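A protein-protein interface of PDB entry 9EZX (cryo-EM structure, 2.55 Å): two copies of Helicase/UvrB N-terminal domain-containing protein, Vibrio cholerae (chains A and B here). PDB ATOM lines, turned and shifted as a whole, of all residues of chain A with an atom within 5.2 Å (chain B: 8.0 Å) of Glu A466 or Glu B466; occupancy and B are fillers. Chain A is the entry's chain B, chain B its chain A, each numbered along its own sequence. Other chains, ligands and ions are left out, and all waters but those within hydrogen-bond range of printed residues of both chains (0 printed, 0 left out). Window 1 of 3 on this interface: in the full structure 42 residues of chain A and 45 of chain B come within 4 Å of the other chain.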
ATOM      1  N   TRP A 298      29.297  -3.270 -18.808  1.00  0.00           N
ATOM      2  CA  TRP A 298      28.750  -3.946 -19.977  1.00  0.00           C
ATOM      3  C   TRP A 298      27.231  -3.968 -19.934  1.00  0.00           C
ATOM      4  O   TRP A 298      26.572  -3.720 -20.948  1.00  0.00           O
ATOM      5  CB  TRP A 298      29.293  -5.369 -20.065  1.00  0.00           C
ATOM      6  CG  TRP A 298      28.539  -6.221 -21.035  1.00  0.00           C
ATOM      7  CD1 TRP A 298      28.789  -6.364 -22.365  1.00  0.00           C
ATOM      8  CD2 TRP A 298      27.399  -7.039 -20.752  1.00  0.00           C
ATOM      9  NE1 TRP A 298      27.879  -7.221 -22.929  1.00  0.00           N
ATOM     10  CE2 TRP A 298      27.014  -7.648 -21.958  1.00  0.00           C
ATOM     11  CE3 TRP A 298      26.666  -7.314 -19.595  1.00  0.00           C
ATOM     12  CZ2 TRP A 298      25.932  -8.518 -22.040  1.00  0.00           C
ATOM     13  CZ3 TRP A 298      25.594  -8.175 -19.679  1.00  0.00           C
ATOM     14  CH2 TRP A 298      25.236  -8.767 -20.892  1.00  0.00           C
ATOM     15  N   THR A 302      24.986  -2.120 -22.758  1.00  0.00           N
ATOM     16  CA  THR A 302      24.083  -2.927 -23.570  1.00  0.00           C
ATOM     17  C   THR A 302      22.645  -2.454 -23.430  1.00  0.00           C
ATOM     18  O   THR A 302      21.925  -2.333 -24.428  1.00  0.00           O
ATOM     19  CB  THR A 302      24.196  -4.395 -23.168  1.00  0.00           C
ATOM     20  OG1 THR A 302      25.561  -4.814 -23.260  1.00  0.00           O
ATOM     21  CG2 THR A 302      23.344  -5.265 -24.068  1.00  0.00           C
ATOM     22  N   ASN A 306      20.515  -0.952 -26.598  1.00  0.00           N
ATOM     23  CA  ASN A 306      19.387  -1.704 -27.128  1.00  0.00           C
ATOM     24  C   ASN A 306      18.054  -1.041 -26.810  1.00  0.00           C
ATOM     25  O   ASN A 306      17.046  -1.340 -27.457  1.00  0.00           O
ATOM     26  CB  ASN A 306      19.420  -3.128 -26.589  1.00  0.00           C
ATOM     27  CG  ASN A 306      20.529  -3.947 -27.199  1.00  0.00           C
ATOM     28  OD1 ASN A 306      20.450  -4.352 -28.356  1.00  0.00           O
ATOM     29  ND2 ASN A 306      21.579  -4.185 -26.430  1.00  0.00           N
ATOM     30  N   ASN A 463      16.097  -7.145 -28.161  1.00  0.00           N
ATOM     31  CA  ASN A 463      17.429  -7.629 -28.513  1.00  0.00           C
ATOM     32  C   ASN A 463      18.311  -7.786 -27.280  1.00  0.00           C
ATOM     33  O   ASN A 463      19.530  -7.622 -27.350  1.00  0.00           O
ATOM     34  CB  ASN A 463      18.101  -6.702 -29.526  1.00  0.00           C
ATOM     35  CG  ASN A 463      19.146  -7.409 -30.354  1.00  0.00           C
ATOM     36  OD1 ASN A 463      18.846  -8.363 -31.068  1.00  0.00           O
ATOM     37  ND2 ASN A 463      20.383  -6.946 -30.266  1.00  0.00           N
ATOM     38  N   LEU A 464      17.702  -8.109 -26.141  1.00  0.00           N
ATOM     39  CA  LEU A 464      18.413  -8.265 -24.880  1.00  0.00           C
ATOM     40  C   LEU A 464      18.487  -9.725 -24.451  1.00  0.00           C
ATOM     41  O   LEU A 464      18.410 -10.032 -23.261  1.00  0.00           O
ATOM     42  CB  LEU A 464      17.749  -7.423 -23.794  1.00  0.00           C
ATOM     43  CG  LEU A 464      17.823  -5.913 -24.007  1.00  0.00           C
ATOM     44  CD1 LEU A 464      16.823  -5.200 -23.126  1.00  0.00           C
ATOM     45  CD2 LEU A 464      19.222  -5.408 -23.733  1.00  0.00           C
ATOM     46  N   GLN A 465      18.641 -10.638 -25.411  1.00  0.00           N
ATOM     47  CA  GLN A 465      18.687 -12.055 -25.078  1.00  0.00           C
ATOM     48  C   GLN A 465      19.835 -12.375 -24.132  1.00  0.00           C
ATOM     49  O   GLN A 465      19.779 -13.370 -23.403  1.00  0.00           O
ATOM     50  CB  GLN A 465      18.808 -12.889 -26.353  1.00  0.00           C
ATOM     51  CG  GLN A 465      17.608 -12.786 -27.273  1.00  0.00           C
ATOM     52  CD  GLN A 465      17.837 -11.830 -28.421  1.00  0.00           C
ATOM     53  OE1 GLN A 465      18.437 -10.772 -28.250  1.00  0.00           O
ATOM     54  NE2 GLN A 465      17.359 -12.198 -29.602  1.00  0.00           N
ATOM     55  N   GLU A 466      20.882 -11.549 -24.129  1.00  0.00           N
ATOM     56  CA  GLU A 466      22.020 -11.801 -23.252  1.00  0.00           C
ATOM     57  C   GLU A 466      21.645 -11.696 -21.781  1.00  0.00           C
ATOM     58  O   GLU A 466      22.374 -12.213 -20.929  1.00  0.00           O
ATOM     59  CB  GLU A 466      23.169 -10.835 -23.555  1.00  0.00           C
ATOM     60  CG  GLU A 466      22.755  -9.415 -23.924  1.00  0.00           C
ATOM     61  CD  GLU A 466      22.466  -9.248 -25.404  1.00  0.00           C
ATOM     62  OE1 GLU A 466      22.550  -8.109 -25.907  1.00  0.00           O
ATOM     63  OE2 GLU A 466      22.153 -10.260 -26.066  1.00  0.00           O
ATOM     64  N   PHE A 467      20.533 -11.041 -21.463  1.00  0.00           N
ATOM     65  CA  PHE A 467      20.068 -10.914 -20.090  1.00  0.00           C
ATOM     66  C   PHE A 467      19.118 -12.030 -19.683  1.00  0.00           C
ATOM     67  O   PHE A 467      18.538 -11.963 -18.596  1.00  0.00           O
ATOM     68  CB  PHE A 467      19.376  -9.564 -19.892  1.00  0.00           C
ATOM     69  CG  PHE A 467      20.319  -8.402 -19.867  1.00  0.00           C
ATOM     70  CD1 PHE A 467      21.022  -8.091 -18.720  1.00  0.00           C
ATOM     71  CD2 PHE A 467      20.502  -7.618 -20.988  1.00  0.00           C
ATOM     72  CE1 PHE A 467      21.888  -7.024 -18.693  1.00  0.00           C
ATOM     73  CE2 PHE A 467      21.367  -6.548 -20.964  1.00  0.00           C
ATOM     74  CZ  PHE A 467      22.060  -6.251 -19.817  1.00  0.00           C
ATOM     75  N   GLU A 468      18.942 -13.048 -20.524  1.00  0.00           N
ATOM     76  CA  GLU A 468      18.006 -14.122 -20.210  1.00  0.00           C
ATOM     77  C   GLU A 468      18.360 -14.788 -18.888  1.00  0.00           C
ATOM     78  O   GLU A 468      17.494 -14.999 -18.033  1.00  0.00           O
ATOM     79  CB  GLU A 468      17.996 -15.144 -21.346  1.00  0.00           C
ATOM     80  CG  GLU A 468      16.980 -16.259 -21.182  1.00  0.00           C
ATOM     81  CD  GLU A 468      17.308 -17.466 -22.036  1.00  0.00           C
ATOM     82  OE1 GLU A 468      17.402 -17.313 -23.272  1.00  0.00           O
ATOM     83  OE2 GLU A 468      17.478 -18.567 -21.473  1.00  0.00           O
ATOM     84  N   SER A 469      19.637 -15.127 -18.703  1.00  0.00           N
ATOM     85  CA  SER A 469      20.048 -15.796 -17.474  1.00  0.00           C
ATOM     86  C   SER A 469      19.782 -14.919 -16.259  1.00  0.00           C
ATOM     87  O   SER A 469      19.257 -15.387 -15.245  1.00  0.00           O
ATOM     88  CB  SER A 469      21.529 -16.163 -17.554  1.00  0.00           C
ATOM     89  OG  SER A 469      21.814 -16.852 -18.757  1.00  0.00           O
ATOM     90  N   GLN B 294      24.745 -18.696 -36.839  1.00  0.00           N
ATOM     91  CA  GLN B 294      24.521 -17.363 -36.303  1.00  0.00           C
ATOM     92  C   GLN B 294      23.104 -16.900 -36.602  1.00  0.00           C
ATOM     93  O   GLN B 294      22.562 -17.181 -37.675  1.00  0.00           O
ATOM     94  CB  GLN B 294      25.515 -16.362 -36.891  1.00  0.00           C
ATOM     95  CG  GLN B 294      26.733 -16.135 -36.029  1.00  0.00           C
ATOM     96  CD  GLN B 294      26.467 -15.169 -34.896  1.00  0.00           C
ATOM     97  OE1 GLN B 294      25.333 -15.021 -34.446  1.00  0.00           O
ATOM     98  NE2 GLN B 294      27.515 -14.506 -34.426  1.00  0.00           N
ATOM     99  N   TRP B 298      19.674 -11.059 -34.917  1.00  0.00           N
ATOM    100  CA  TRP B 298      20.286 -10.637 -33.665  1.00  0.00           C
ATOM    101  C   TRP B 298      21.662 -10.037 -33.903  1.00  0.00           C
ATOM    102  O   TRP B 298      22.006  -9.007 -33.317  1.00  0.00           O
ATOM    103  CB  TRP B 298      20.388 -11.819 -32.703  1.00  0.00           C
ATOM    104  CG  TRP B 298      21.301 -11.554 -31.549  1.00  0.00           C
ATOM    105  CD1 TRP B 298      20.966 -10.999 -30.352  1.00  0.00           C
ATOM    106  CD2 TRP B 298      22.706 -11.820 -31.487  1.00  0.00           C
ATOM    107  NE1 TRP B 298      22.072 -10.906 -29.546  1.00  0.00           N
ATOM    108  CE2 TRP B 298      23.154 -11.403 -30.222  1.00  0.00           C
ATOM    109  CE3 TRP B 298      23.629 -12.371 -32.380  1.00  0.00           C
ATOM    110  CZ2 TRP B 298      24.482 -11.521 -29.826  1.00  0.00           C
ATOM    111  CZ3 TRP B 298      24.945 -12.486 -31.985  1.00  0.00           C
ATOM    112  CH2 TRP B 298      25.360 -12.063 -30.721  1.00  0.00           C
ATOM    113  N   THR B 302      22.496  -6.179 -32.996  1.00  0.00           N
ATOM    114  CA  THR B 302      23.528  -5.898 -32.006  1.00  0.00           C
ATOM    115  C   THR B 302      24.633  -5.035 -32.593  1.00  0.00           C
ATOM    116  O   THR B 302      25.081  -4.070 -31.961  1.00  0.00           O
ATOM    117  CB  THR B 302      24.109  -7.208 -31.476  1.00  0.00           C
ATOM    118  OG1 THR B 302      23.050  -8.040 -30.992  1.00  0.00           O
ATOM    119  CG2 THR B 302      25.093  -6.945 -30.356  1.00  0.00           C
ATOM    120  N   LEU B 303      25.067  -5.356 -33.814  1.00  0.00           N
ATOM    121  CA  LEU B 303      26.143  -4.595 -34.495  1.00  0.00           C
ATOM    122  C   LEU B 303      25.642  -3.182 -34.785  1.00  0.00           C
ATOM    123  O   LEU B 303      26.397  -2.279 -34.545  1.00  0.00           O
ATOM    124  CB  LEU B 303      26.577  -5.306 -35.782  1.00  0.00           C
ATOM    125  CG  LEU B 303      27.446  -6.550 -35.594  1.00  0.00           C
ATOM    126  CD1 LEU B 303      27.428  -7.425 -36.840  1.00  0.00           C
ATOM    127  CD2 LEU B 303      28.876  -6.179 -35.231  1.00  0.00           C
ATOM    128  N   ASN B 306      25.420  -1.260 -31.180  1.00  0.00           N
ATOM    129  CA  ASN B 306      26.667  -0.994 -30.476  1.00  0.00           C
ATOM    130  C   ASN B 306      27.607  -0.114 -31.288  1.00  0.00           C
ATOM    131  O   ASN B 306      28.450   0.582 -30.714  1.00  0.00           O
ATOM    132  CB  ASN B 306      27.342  -2.312 -30.114  1.00  0.00           C
ATOM    133  CG  ASN B 306      26.619  -3.041 -29.009  1.00  0.00           C
ATOM    134  OD1 ASN B 306      26.696  -2.659 -27.845  1.00  0.00           O
ATOM    135  ND2 ASN B 306      25.898  -4.091 -29.369  1.00  0.00           N
ATOM    136  N   TYR B 416      27.637  -9.002 -41.972  1.00  0.00           N
ATOM    137  CA  TYR B 416      28.252  -9.789 -40.906  1.00  0.00           C
ATOM    138  C   TYR B 416      29.655 -10.245 -41.293  1.00  0.00           C
ATOM    139  O   TYR B 416      30.603 -10.117 -40.503  1.00  0.00           O
ATOM    140  CB  TYR B 416      27.362 -10.985 -40.580  1.00  0.00           C
ATOM    141  CG  TYR B 416      27.897 -11.879 -39.492  1.00  0.00           C
ATOM    142  CD1 TYR B 416      28.041 -11.414 -38.196  1.00  0.00           C
ATOM    143  CD2 TYR B 416      28.246 -13.191 -39.758  1.00  0.00           C
ATOM    144  CE1 TYR B 416      28.522 -12.227 -37.201  1.00  0.00           C
ATOM    145  CE2 TYR B 416      28.731 -14.011 -38.768  1.00  0.00           C
ATOM    146  CZ  TYR B 416      28.867 -13.526 -37.492  1.00  0.00           C
ATOM    147  OH  TYR B 416      29.351 -14.344 -36.500  1.00  0.00           O
ATOM    148  N   PHE B 419      31.928  -7.352 -41.097  1.00  0.00           N
ATOM    149  CA  PHE B 419      32.348  -7.077 -39.730  1.00  0.00           C
ATOM    150  C   PHE B 419      33.480  -8.003 -39.315  1.00  0.00           C
ATOM    151  O   PHE B 419      34.462  -7.568 -38.709  1.00  0.00           O
ATOM    152  CB  PHE B 419      31.165  -7.225 -38.777  1.00  0.00           C
ATOM    153  CG  PHE B 419      31.566  -7.367 -37.340  1.00  0.00           C
ATOM    154  CD1 PHE B 419      32.149  -6.314 -36.663  1.00  0.00           C
ATOM    155  CD2 PHE B 419      31.367  -8.557 -36.667  1.00  0.00           C
ATOM    156  CE1 PHE B 419      32.521  -6.444 -35.344  1.00  0.00           C
ATOM    157  CE2 PHE B 419      31.737  -8.690 -35.349  1.00  0.00           C
ATOM    158  CZ  PHE B 419      32.314  -7.633 -34.687  1.00  0.00           C
ATOM    159  N   LEU B 459      36.725  -5.693 -29.033  1.00  0.00           N
ATOM    160  CA  LEU B 459      35.354  -6.055 -28.699  1.00  0.00           C
ATOM    161  C   LEU B 459      34.884  -5.335 -27.443  1.00  0.00           C
ATOM    162  O   LEU B 459      33.731  -4.898 -27.366  1.00  0.00           O
ATOM    163  CB  LEU B 459      35.237  -7.569 -28.531  1.00  0.00           C
ATOM    164  CG  LEU B 459      35.416  -8.397 -29.804  1.00  0.00           C
ATOM    165  CD1 LEU B 459      35.158  -9.857 -29.512  1.00  0.00           C
ATOM    166  CD2 LEU B 459      34.509  -7.915 -30.919  1.00  0.00           C
ATOM    167  N   THR B 460      35.760  -5.195 -26.447  1.00  0.00           N
ATOM    168  CA  THR B 460      35.366  -4.530 -25.211  1.00  0.00           C
ATOM    169  C   THR B 460      35.082  -3.052 -25.443  1.00  0.00           C
ATOM    170  O   THR B 460      34.132  -2.503 -24.879  1.00  0.00           O
ATOM    171  CB  THR B 460      36.452  -4.704 -24.153  1.00  0.00           C
ATOM    172  OG1 THR B 460      36.832  -6.083 -24.083  1.00  0.00           O
ATOM    173  CG2 THR B 460      35.946  -4.268 -22.799  1.00  0.00           C
ATOM    174  N   PHE B 462      33.991  -1.597 -28.164  1.00  0.00           N
ATOM    175  CA  PHE B 462      32.723  -1.475 -28.868  1.00  0.00           C
ATOM    176  C   PHE B 462      31.567  -2.136 -28.134  1.00  0.00           C
ATOM    177  O   PHE B 462      30.426  -2.014 -28.584  1.00  0.00           O
ATOM    178  CB  PHE B 462      32.835  -2.086 -30.265  1.00  0.00           C
ATOM    179  CG  PHE B 462      33.791  -1.369 -31.168  1.00  0.00           C
ATOM    180  CD1 PHE B 462      33.713   0.000 -31.336  1.00  0.00           C
ATOM    181  CD2 PHE B 462      34.762  -2.067 -31.861  1.00  0.00           C
ATOM    182  CE1 PHE B 462      34.589   0.657 -32.168  1.00  0.00           C
ATOM    183  CE2 PHE B 462      35.638  -1.414 -32.694  1.00  0.00           C
ATOM    184  CZ  PHE B 462      35.550  -0.051 -32.849  1.00  0.00           C
ATOM    185  N   ASN B 463      31.828  -2.826 -27.027  1.00  0.00           N
ATOM    186  CA  ASN B 463      30.782  -3.509 -26.271  1.00  0.00           C
ATOM    187  C   ASN B 463      30.213  -4.682 -27.064  1.00  0.00           C
ATOM    188  O   ASN B 463      29.034  -5.018 -26.954  1.00  0.00           O
ATOM    189  CB  ASN B 463      29.671  -2.539 -25.870  1.00  0.00           C
ATOM    190  CG  ASN B 463      28.836  -3.055 -24.722  1.00  0.00           C
ATOM    191  OD1 ASN B 463      29.317  -3.176 -23.599  1.00  0.00           O
ATOM    192  ND2 ASN B 463      27.578  -3.358 -24.998  1.00  0.00           N
ATOM    193  N   LEU B 464      31.064  -5.313 -27.870  1.00  0.00           N
ATOM    194  CA  LEU B 464      30.672  -6.434 -28.712  1.00  0.00           C
ATOM    195  C   LEU B 464      31.282  -7.744 -28.225  1.00  0.00           C
ATOM    196  O   LEU B 464      31.691  -8.581 -29.029  1.00  0.00           O
ATOM    197  CB  LEU B 464      31.070  -6.169 -30.161  1.00  0.00           C
ATOM    198  CG  LEU B 464      30.303  -5.040 -30.847  1.00  0.00           C
ATOM    199  CD1 LEU B 464      31.012  -4.605 -32.107  1.00  0.00           C
ATOM    200  CD2 LEU B 464      28.887  -5.474 -31.158  1.00  0.00           C
ATOM    201  N   GLN B 465      31.341  -7.936 -26.907  1.00  0.00           N
ATOM    202  CA  GLN B 465      31.916  -9.159 -26.364  1.00  0.00           C
ATOM    203  C   GLN B 465      31.121 -10.392 -26.766  1.00  0.00           C
ATOM    204  O   GLN B 465      31.629 -11.511 -26.644  1.00  0.00           O
ATOM    205  CB  GLN B 465      31.995  -9.070 -24.841  1.00  0.00           C
ATOM    206  CG  GLN B 465      32.934  -7.995 -24.335  1.00  0.00           C
ATOM    207  CD  GLN B 465      32.203  -6.750 -23.885  1.00  0.00           C
ATOM    208  OE1 GLN B 465      31.256  -6.307 -24.530  1.00  0.00           O
ATOM    209  NE2 GLN B 465      32.640  -6.175 -22.773  1.00  0.00           N
ATOM    210  N   GLU B 466      29.888 -10.215 -27.242  1.00  0.00           N
ATOM    211  CA  GLU B 466      29.084 -11.360 -27.650  1.00  0.00           C
ATOM    212  C   GLU B 466      29.663 -12.040 -28.881  1.00  0.00           C
ATOM    213  O   GLU B 466      29.400 -13.224 -29.116  1.00  0.00           O
ATOM    214  CB  GLU B 466      27.640 -10.933 -27.922  1.00  0.00           C
ATOM    215  CG  GLU B 466      26.942 -10.195 -26.777  1.00  0.00           C
ATOM    216  CD  GLU B 466      27.363  -8.742 -26.643  1.00  0.00           C
ATOM    217  OE1 GLU B 466      28.581  -8.476 -26.577  1.00  0.00           O
ATOM    218  OE2 GLU B 466      26.477  -7.865 -26.605  1.00  0.00           O
ATOM    219  N   PHE B 467      30.449 -11.317 -29.673  1.00  0.00           N
ATOM    220  CA  PHE B 467      31.019 -11.842 -30.904  1.00  0.00           C
ATOM    221  C   PHE B 467      32.405 -12.436 -30.710  1.00  0.00           C
ATOM    222  O   PHE B 467      33.068 -12.756 -31.701  1.00  0.00           O
ATOM    223  CB  PHE B 467      31.086 -10.738 -31.960  1.00  0.00           C
ATOM    224  CG  PHE B 467      29.745 -10.309 -32.469  1.00  0.00           C
ATOM    225  CD1 PHE B 467      29.100 -11.034 -33.451  1.00  0.00           C
ATOM    226  CD2 PHE B 467      29.132  -9.178 -31.969  1.00  0.00           C
ATOM    227  CE1 PHE B 467      27.868 -10.640 -33.920  1.00  0.00           C
ATOM    228  CE2 PHE B 467      27.900  -8.782 -32.437  1.00  0.00           C
ATOM    229  CZ  PHE B 467      27.269  -9.513 -33.413  1.00  0.00           C
ATOM    230  N   GLU B 468      32.862 -12.589 -29.468  1.00  0.00           N
ATOM    231  CA  GLU B 468      34.201 -13.113 -29.230  1.00  0.00           C
ATOM    232  C   GLU B 468      34.357 -14.503 -29.832  1.00  0.00           C
ATOM    233  O   GLU B 468      35.354 -14.796 -30.502  1.00  0.00           O
ATOM    234  CB  GLU B 468      34.485 -13.134 -27.729  1.00  0.00           C
ATOM    235  CG  GLU B 468      35.870 -13.632 -27.348  1.00  0.00           C
ATOM    236  CD  GLU B 468      35.924 -14.147 -25.925  1.00  0.00           C
ATOM    237  OE1 GLU B 468      36.280 -15.328 -25.730  1.00  0.00           O
ATOM    238  OE2 GLU B 468      35.609 -13.370 -25.001  1.00  0.00           O
ATOM    239  N   SER B 469      33.374 -15.375 -29.607  1.00  0.00           N
ATOM    240  CA  SER B 469      33.453 -16.730 -30.141  1.00  0.00           C
ATOM    241  C   SER B 469      33.470 -16.716 -31.662  1.00  0.00           C
ATOM    242  O   SER B 469      34.235 -17.454 -32.294  1.00  0.00           O
ATOM    243  CB  SER B 469      32.278 -17.560 -29.626  1.00  0.00           C
ATOM    244  OG  SER B 469      32.127 -17.408 -28.227  1.00  0.00           O
ATOM    245  N   ALA B 470      32.629 -15.881 -32.271  1.00  0.00           N
ATOM    246  CA  ALA B 470      32.568 -15.825 -33.727  1.00  0.00           C
ATOM    247  C   ALA B 470      33.892 -15.359 -34.316  1.00  0.00           C
ATOM    248  O   ALA B 470      34.341 -15.882 -35.342  1.00  0.00           O
ATOM    249  CB  ALA B 470      31.433 -14.904 -34.166  1.00  0.00           C
ATOM    250  N   VAL B 471      34.525 -14.368 -33.689  1.00  0.00           N
ATOM    251  CA  VAL B 471      35.780 -13.839 -34.217  1.00  0.00           C
ATOM    252  C   VAL B 471      36.878 -14.892 -34.132  1.00  0.00           C
ATOM    253  O   VAL B 471      37.635 -15.102 -35.086  1.00  0.00           O
ATOM    254  CB  VAL B 471      36.174 -12.552 -33.473  1.00  0.00           C
ATOM    255  CG1 VAL B 471      37.580 -12.126 -33.860  1.00  0.00           C
ATOM    256  CG2 VAL B 471      35.179 -11.445 -33.769  1.00  0.00           C
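The side-chain amide nitrogen of Asn A463 is in hydrogen-bond range of the side-chain hydroxyl of Thr B302, at 3.0 Å. The side-chain hydroxyl (OG1) of Thr A302 is in hydrogen-bond range of the side-chain amide nitrogen (ND2) of Asn B463, at 3.0 Å.
O of Trp B298 sits at hydrogen-bond distance from OG1 of Thr B302 (2.7 Å). ND2 of Asn B306 is in hydrogen-bond range of O of Thr B302 (2.7 Å). The side-chain amide nitrogen of Asn B463 is in hydrogen-bond range of the side-chain amide oxygen of Asn B306 (3.1 Å). O of Trp A298 is in hydrogen-bond range of OG1 of Thr A302 (2.8 Å). ND2 of Asn A306 lies within hydrogen-bond range of O of Thr A302. O of Asn A463 sits close to OE1 of Gln A465 (3.5 Å).
Among the printed residues, pairs that only touch across the chains: Trp A298 with Gln B465, Gln A465 with Trp B298, Asn A463 with Trp B298, Trp A298 with Asn B463, Glu A466 with Trp B298, Trp A298 with Glu B466 and Glu A466 with Glu B466.
Of the printed residues of chain B, Glu A466 touches Trp B298 and Glu B466. Of the printed residues of chain A, Glu B466 touches Trp A298 (3.9 Å) and Glu A466 (3.996 Å). Of the printed residues of chain A, Gln B465 touches Trp A298 (3.3 Å). Printed residues of chain B within 4 Å of Thr A302: Asn B463. Printed residues of chain B within 4 Å of Gln A465: Trp B298. Of the printed residues of chain B, Asn A463 touches Trp B298 and Thr B302. Printed residues of chain A within 4 Å of Thr B302: Asn A463 (3.0 Å). Asn B306 touches none of the printed residues of chain A. Tyr B416 touches none of the printed residues of chain A. The nearest printed residue of chain B that does not touch Glu A466 is Thr B302 (5.1 Å). The nearest printed residue of chain A that does not touch Asn B463 is Asn A306 (6.2 Å).
Printed residues of chain A that touch a printed residue of chain B: Trp A298, Thr A302, Asn A463, Gln A465 and Glu A466. Along chain A the printed residues that touch a printed residue of chain B span positions 298 to 466. Among the printed residues, 9 pairs touch across the chains. Among the printed residues, no Asp or Glu carboxylate lies within 4 Å of a Lys or Arg side-chain nitrogen of the other chain.
Trp A298 touches Gln B465, and with the chains exchanged Gln A465 touches Trp B298. Trp A298 touches Glu B466, and with the chains exchanged Glu A466 touches Trp B298. Thr A302 touches Asn B463, and with the chains exchanged Asn A463 touches Thr B302. Glu B466 touches its own counterpart, Glu A466.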
